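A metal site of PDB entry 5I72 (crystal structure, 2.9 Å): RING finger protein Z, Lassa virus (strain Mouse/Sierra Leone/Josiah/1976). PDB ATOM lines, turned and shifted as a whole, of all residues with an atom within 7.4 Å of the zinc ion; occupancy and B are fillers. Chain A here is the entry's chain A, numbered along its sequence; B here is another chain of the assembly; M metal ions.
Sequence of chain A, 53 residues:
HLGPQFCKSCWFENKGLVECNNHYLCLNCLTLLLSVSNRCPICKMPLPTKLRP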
ATOM      1  N   PHE A   6      26.791 -26.423 -14.325  1.00  0.00           N
ATOM      2  CA  PHE A   6      26.334 -25.799 -15.558  1.00  0.00           C
ATOM      3  C   PHE A   6      25.483 -24.571 -15.249  1.00  0.00           C
ATOM      4  O   PHE A   6      24.787 -24.534 -14.239  1.00  0.00           O
ATOM      5  CB  PHE A   6      25.543 -26.794 -16.419  1.00  0.00           C
ATOM      6  CG  PHE A   6      26.418 -27.679 -17.262  1.00  0.00           C
ATOM      7  CD1 PHE A   6      26.972 -27.207 -18.442  1.00  0.00           C
ATOM      8  CD2 PHE A   6      26.681 -28.989 -16.893  1.00  0.00           C
ATOM      9  CE1 PHE A   6      27.778 -28.024 -19.227  1.00  0.00           C
ATOM     10  CE2 PHE A   6      27.480 -29.808 -17.670  1.00  0.00           C
ATOM     11  CZ  PHE A   6      28.029 -29.321 -18.835  1.00  0.00           C
ATOM     12  N   CYS A   7      25.580 -23.574 -16.113  1.00  0.00           N
ATOM     13  CA  CYS A   7      24.766 -22.366 -15.971  1.00  0.00           C
ATOM     14  C   CYS A   7      23.293 -22.750 -16.078  1.00  0.00           C
ATOM     15  O   CYS A   7      22.858 -23.245 -17.114  1.00  0.00           O
ATOM     16  CB  CYS A   7      25.138 -21.344 -17.052  1.00  0.00           C
ATOM     17  SG  CYS A   7      24.075 -19.883 -17.124  1.00  0.00           S
ATOM     18  N   LYS A   8      22.532 -22.536 -15.009  1.00  0.00           N
ATOM     19  CA  LYS A   8      21.143 -22.993 -14.985  1.00  0.00           C
ATOM     20  C   LYS A   8      20.245 -22.160 -15.901  1.00  0.00           C
ATOM     21  O   LYS A   8      19.077 -22.485 -16.105  1.00  0.00           O
ATOM     22  CB  LYS A   8      20.602 -22.977 -13.543  1.00  0.00           C
ATOM     23  CG  LYS A   8      19.431 -23.943 -13.312  1.00  0.00           C
ATOM     24  CD  LYS A   8      18.899 -23.811 -11.890  1.00  0.00           C
ATOM     25  CE  LYS A   8      17.798 -24.809 -11.594  1.00  0.00           C
ATOM     26  NZ  LYS A   8      17.264 -24.618 -10.208  1.00  0.00           N
ATOM     27  N   SER A   9      20.814 -21.091 -16.462  1.00  0.00           N
ATOM     28  CA  SER A   9      20.070 -20.240 -17.400  1.00  0.00           C
ATOM     29  C   SER A   9      20.210 -20.701 -18.840  1.00  0.00           C
ATOM     30  O   SER A   9      19.214 -20.730 -19.575  1.00  0.00           O
ATOM     31  CB  SER A   9      20.551 -18.793 -17.288  1.00  0.00           C
ATOM     32  OG  SER A   9      20.078 -18.037 -18.393  1.00  0.00           O
ATOM     33  N   CYS A  10      21.419 -21.048 -19.245  1.00  0.00           N
ATOM     34  CA  CYS A  10      21.675 -21.435 -20.626  1.00  0.00           C
ATOM     35  C   CYS A  10      21.989 -22.912 -20.750  1.00  0.00           C
ATOM     36  O   CYS A  10      22.115 -23.428 -21.850  1.00  0.00           O
ATOM     37  CB  CYS A  10      22.820 -20.613 -21.234  1.00  0.00           C
ATOM     38  SG  CYS A  10      24.469 -21.098 -20.652  1.00  0.00           S
ATOM     39  N   TRP A  11      22.122 -23.592 -19.602  1.00  0.00           N
ATOM     40  CA  TRP A  11      22.385 -25.039 -19.554  1.00  0.00           C
ATOM     41  C   TRP A  11      23.501 -25.491 -20.490  1.00  0.00           C
ATOM     42  O   TRP A  11      23.400 -26.559 -21.086  1.00  0.00           O
ATOM     43  CB  TRP A  11      21.107 -25.812 -19.887  1.00  0.00           C
ATOM     44  CG  TRP A  11      20.011 -25.695 -18.857  1.00  0.00           C
ATOM     45  CD1 TRP A  11      19.160 -24.642 -18.677  1.00  0.00           C
ATOM     46  CD2 TRP A  11      19.617 -26.691 -17.910  1.00  0.00           C
ATOM     47  NE1 TRP A  11      18.282 -24.909 -17.656  1.00  0.00           N
ATOM     48  CE2 TRP A  11      18.531 -26.169 -17.171  1.00  0.00           C
ATOM     49  CE3 TRP A  11      20.072 -27.978 -17.611  1.00  0.00           C
ATOM     50  CZ2 TRP A  11      17.908 -26.883 -16.150  1.00  0.00           C
ATOM     51  CZ3 TRP A  11      19.455 -28.680 -16.593  1.00  0.00           C
ATOM     52  CH2 TRP A  11      18.383 -28.129 -15.874  1.00  0.00           C
ATOM     53  N   PHE A  12      24.557 -24.704 -20.610  1.00  0.00           N
ATOM     54  CA  PHE A  12      25.620 -25.055 -21.544  1.00  0.00           C
ATOM     55  C   PHE A  12      27.034 -24.730 -21.054  1.00  0.00           C
ATOM     56  O   PHE A  12      27.933 -25.569 -21.131  1.00  0.00           O
ATOM     57  CB  PHE A  12      25.396 -24.365 -22.879  1.00  0.00           C
ATOM     58  CG  PHE A  12      25.786 -25.195 -24.061  1.00  0.00           C
ATOM     59  CD1 PHE A  12      24.907 -26.141 -24.583  1.00  0.00           C
ATOM     60  CD2 PHE A  12      27.035 -25.055 -24.648  1.00  0.00           C
ATOM     61  CE1 PHE A  12      25.275 -26.912 -25.669  1.00  0.00           C
ATOM     62  CE2 PHE A  12      27.395 -25.824 -25.739  1.00  0.00           C
ATOM     63  CZ  PHE A  12      26.519 -26.757 -26.240  1.00  0.00           C
ATOM     64  N   GLU A  13      27.230 -23.509 -20.556  1.00  0.00           N
ATOM     65  CA  GLU A  13      28.557 -23.082 -20.107  1.00  0.00           C
ATOM     66  C   GLU A  13      28.938 -23.736 -18.787  1.00  0.00           C
ATOM     67  O   GLU A  13      28.155 -23.756 -17.832  1.00  0.00           O
ATOM     68  CB  GLU A  13      28.622 -21.564 -19.979  1.00  0.00           C
ATOM     69  CG  GLU A  13      30.043 -21.061 -19.808  1.00  0.00           C
ATOM     70  CD  GLU A  13      30.906 -21.383 -21.003  1.00  0.00           C
ATOM     71  OE1 GLU A  13      31.628 -22.401 -20.954  1.00  0.00           O
ATOM     72  OE2 GLU A  13      30.873 -20.624 -21.995  1.00  0.00           O
ATOM     73  N   LEU A  17      32.065 -19.832 -14.121  1.00  0.00           N
ATOM     74  CA  LEU A  17      30.769 -19.883 -13.477  1.00  0.00           C
ATOM     75  C   LEU A  17      30.776 -19.135 -12.152  1.00  0.00           C
ATOM     76  O   LEU A  17      31.662 -19.316 -11.311  1.00  0.00           O
ATOM     77  CB  LEU A  17      30.338 -21.328 -13.214  1.00  0.00           C
ATOM     78  CG  LEU A  17      29.996 -22.190 -14.432  1.00  0.00           C
ATOM     79  CD1 LEU A  17      29.609 -23.599 -13.980  1.00  0.00           C
ATOM     80  CD2 LEU A  17      28.876 -21.553 -15.224  1.00  0.00           C
ATOM     81  N   TYR A  24      24.132 -22.294 -10.586  1.00  0.00           N
ATOM     82  CA  TYR A  24      25.236 -21.562 -11.205  1.00  0.00           C
ATOM     83  C   TYR A  24      24.763 -20.624 -12.302  1.00  0.00           C
ATOM     84  O   TYR A  24      23.650 -20.724 -12.793  1.00  0.00           O
ATOM     85  CB  TYR A  24      26.274 -22.544 -11.774  1.00  0.00           C
ATOM     86  CG  TYR A  24      26.995 -23.350 -10.730  1.00  0.00           C
ATOM     87  CD1 TYR A  24      27.996 -22.764  -9.949  1.00  0.00           C
ATOM     88  CD2 TYR A  24      26.691 -24.690 -10.511  1.00  0.00           C
ATOM     89  CE1 TYR A  24      28.675 -23.500  -8.987  1.00  0.00           C
ATOM     90  CE2 TYR A  24      27.362 -25.432  -9.558  1.00  0.00           C
ATOM     91  CZ  TYR A  24      28.354 -24.837  -8.796  1.00  0.00           C
ATOM     92  OH  TYR A  24      29.018 -25.567  -7.845  1.00  0.00           O
ATOM     93  N   LEU A  25      25.647 -19.694 -12.675  1.00  0.00           N
ATOM     94  CA  LEU A  25      25.411 -18.798 -13.798  1.00  0.00           C
ATOM     95  C   LEU A  25      26.727 -18.466 -14.493  1.00  0.00           C
ATOM     96  O   LEU A  25      27.712 -18.119 -13.837  1.00  0.00           O
ATOM     97  CB  LEU A  25      24.722 -17.506 -13.338  1.00  0.00           C
ATOM     98  CG  LEU A  25      23.219 -17.542 -13.077  1.00  0.00           C
ATOM     99  CD1 LEU A  25      22.744 -16.190 -12.573  1.00  0.00           C
ATOM    100  CD2 LEU A  25      22.477 -17.924 -14.343  1.00  0.00           C
ATOM    101  N   CYS A  26      26.744 -18.562 -15.819  1.00  0.00           N
ATOM    102  CA  CYS A  26      27.905 -18.154 -16.583  1.00  0.00           C
ATOM    103  C   CYS A  26      27.952 -16.630 -16.620  1.00  0.00           C
ATOM    104  O   CYS A  26      26.957 -15.974 -16.319  1.00  0.00           O
ATOM    105  CB  CYS A  26      27.865 -18.729 -18.000  1.00  0.00           C
ATOM    106  SG  CYS A  26      26.591 -18.013 -19.053  1.00  0.00           S
ATOM    107  N   LEU A  27      29.099 -16.073 -16.986  1.00  0.00           N
ATOM    108  CA  LEU A  27      29.289 -14.634 -16.927  1.00  0.00           C
ATOM    109  C   LEU A  27      28.336 -13.876 -17.861  1.00  0.00           C
ATOM    110  O   LEU A  27      27.785 -12.845 -17.481  1.00  0.00           O
ATOM    111  CB  LEU A  27      30.732 -14.267 -17.265  1.00  0.00           C
ATOM    112  CG  LEU A  27      31.277 -13.065 -16.508  1.00  0.00           C
ATOM    113  CD1 LEU A  27      31.588 -13.447 -15.072  1.00  0.00           C
ATOM    114  CD2 LEU A  27      32.502 -12.497 -17.201  1.00  0.00           C
ATOM    115  N   ASN A  28      28.145 -14.397 -19.064  1.00  0.00           N
ATOM    116  CA  ASN A  28      27.274 -13.765 -20.052  1.00  0.00           C
ATOM    117  C   ASN A  28      25.820 -13.685 -19.583  1.00  0.00           C
ATOM    118  O   ASN A  28      25.169 -12.654 -19.703  1.00  0.00           O
ATOM    119  CB  ASN A  28      27.358 -14.495 -21.386  1.00  0.00           C
ATOM    120  CG  ASN A  28      28.760 -14.504 -21.958  1.00  0.00           C
ATOM    121  OD1 ASN A  28      29.156 -13.586 -22.669  1.00  0.00           O
ATOM    122  ND2 ASN A  28      29.517 -15.547 -21.653  1.00  0.00           N
ATOM    123  N   CYS A  29      25.324 -14.801 -19.056  1.00  0.00           N
ATOM    124  CA  CYS A  29      23.962 -14.876 -18.548  1.00  0.00           C
ATOM    125  C   CYS A  29      23.763 -13.961 -17.347  1.00  0.00           C
ATOM    126  O   CYS A  29      22.761 -13.250 -17.253  1.00  0.00           O
ATOM    127  CB  CYS A  29      23.598 -16.311 -18.194  1.00  0.00           C
ATOM    128  SG  CYS A  29      23.324 -17.371 -19.627  1.00  0.00           S
ATOM    129  N   LEU A  30      24.720 -13.983 -16.429  1.00  0.00           N
ATOM    130  CA  LEU A  30      24.660 -13.145 -15.229  1.00  0.00           C
ATOM    131  C   LEU A  30      24.568 -11.665 -15.596  1.00  0.00           C
ATOM    132  O   LEU A  30      23.819 -10.915 -14.977  1.00  0.00           O
ATOM    133  CB  LEU A  30      25.884 -13.383 -14.345  1.00  0.00           C
ATOM    134  CG  LEU A  30      26.043 -12.491 -13.111  1.00  0.00           C
ATOM    135  CD1 LEU A  30      24.763 -12.466 -12.289  1.00  0.00           C
ATOM    136  CD2 LEU A  30      27.217 -12.967 -12.271  1.00  0.00           C
ATOM    137  N   LEU B  32      21.648 -14.614 -27.251  1.00  0.00           N
ATOM    138  CA  LEU B  32      22.570 -15.297 -26.359  1.00  0.00           C
ATOM    139  C   LEU B  32      22.404 -16.808 -26.435  1.00  0.00           C
ATOM    140  O   LEU B  32      23.380 -17.550 -26.370  1.00  0.00           O
ATOM    141  CB  LEU B  32      22.374 -14.819 -24.921  1.00  0.00           C
ATOM    142  CG  LEU B  32      23.289 -15.442 -23.863  1.00  0.00           C
ATOM    143  CD1 LEU B  32      24.754 -15.360 -24.279  1.00  0.00           C
ATOM    144  CD2 LEU B  32      23.075 -14.759 -22.522  1.00  0.00           C
ATOM    145  N   LEU B  33      21.165 -17.265 -26.596  1.00  0.00           N
ATOM    146  CA  LEU B  33      20.885 -18.688 -26.702  1.00  0.00           C
ATOM    147  C   LEU B  33      21.383 -19.274 -28.021  1.00  0.00           C
ATOM    148  O   LEU B  33      21.892 -20.391 -28.056  1.00  0.00           O
ATOM    149  CB  LEU B  33      19.384 -18.956 -26.533  1.00  0.00           C
ATOM    150  CG  LEU B  33      18.798 -18.625 -25.159  1.00  0.00           C
ATOM    151  CD1 LEU B  33      17.294 -18.822 -25.160  1.00  0.00           C
ATOM    152  CD2 LEU B  33      19.444 -19.476 -24.073  1.00  0.00           C
ATOM    153  N   VAL B  36      24.939 -20.143 -28.206  1.00  0.00           N
ATOM    154  CA  VAL B  36      25.386 -21.335 -27.510  1.00  0.00           C
ATOM    155  C   VAL B  36      24.944 -22.625 -28.207  1.00  0.00           C
ATOM    156  O   VAL B  36      25.688 -23.608 -28.222  1.00  0.00           O
ATOM    157  CB  VAL B  36      24.862 -21.322 -26.040  1.00  0.00           C
ATOM    158  CG1 VAL B  36      24.154 -22.615 -25.692  1.00  0.00           C
ATOM    159  CG2 VAL B  36      26.007 -21.043 -25.073  1.00  0.00           C
HETATM  160 ZN    ZN M   1      24.625 -19.263 -19.329  1.00  0.00          ZN
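The backbone NH (N) of Ser 9 lies close to the side-chain sulfur (SG) of Cys 7. The backbone NH (N) of Phe 12 lies close to the side-chain sulfur (SG) of Cys 10. The backbone carbonyl oxygen (O) of Glu 13 lies within hydrogen-bond range of the backbone NH (N) of Cys 7 (3.1 Å). SG of Cys 10 sits close to N of Glu 13, 3.7 Å away. The side-chain sulfur (SG) of Cys 29 sits close to the side-chain hydroxyl (OG) of Ser 9, at 3.5 Å.
SG of Cys 10 binds the zinc ion (2.3 Å). The zinc ion is bound by SG of Cys 29, at 2.3 Å. The zinc ion is bound by the side-chain sulfur (SG) of Cys 26, 2.3 Å away. SG of Cys 7 is bound to the zinc ion (2.4 Å). The zinc ion has four donor atoms within binding distance.
Within 4 Å of the zinc ion: Cys 7, Cys 10, Cys 26 and Cys 29.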
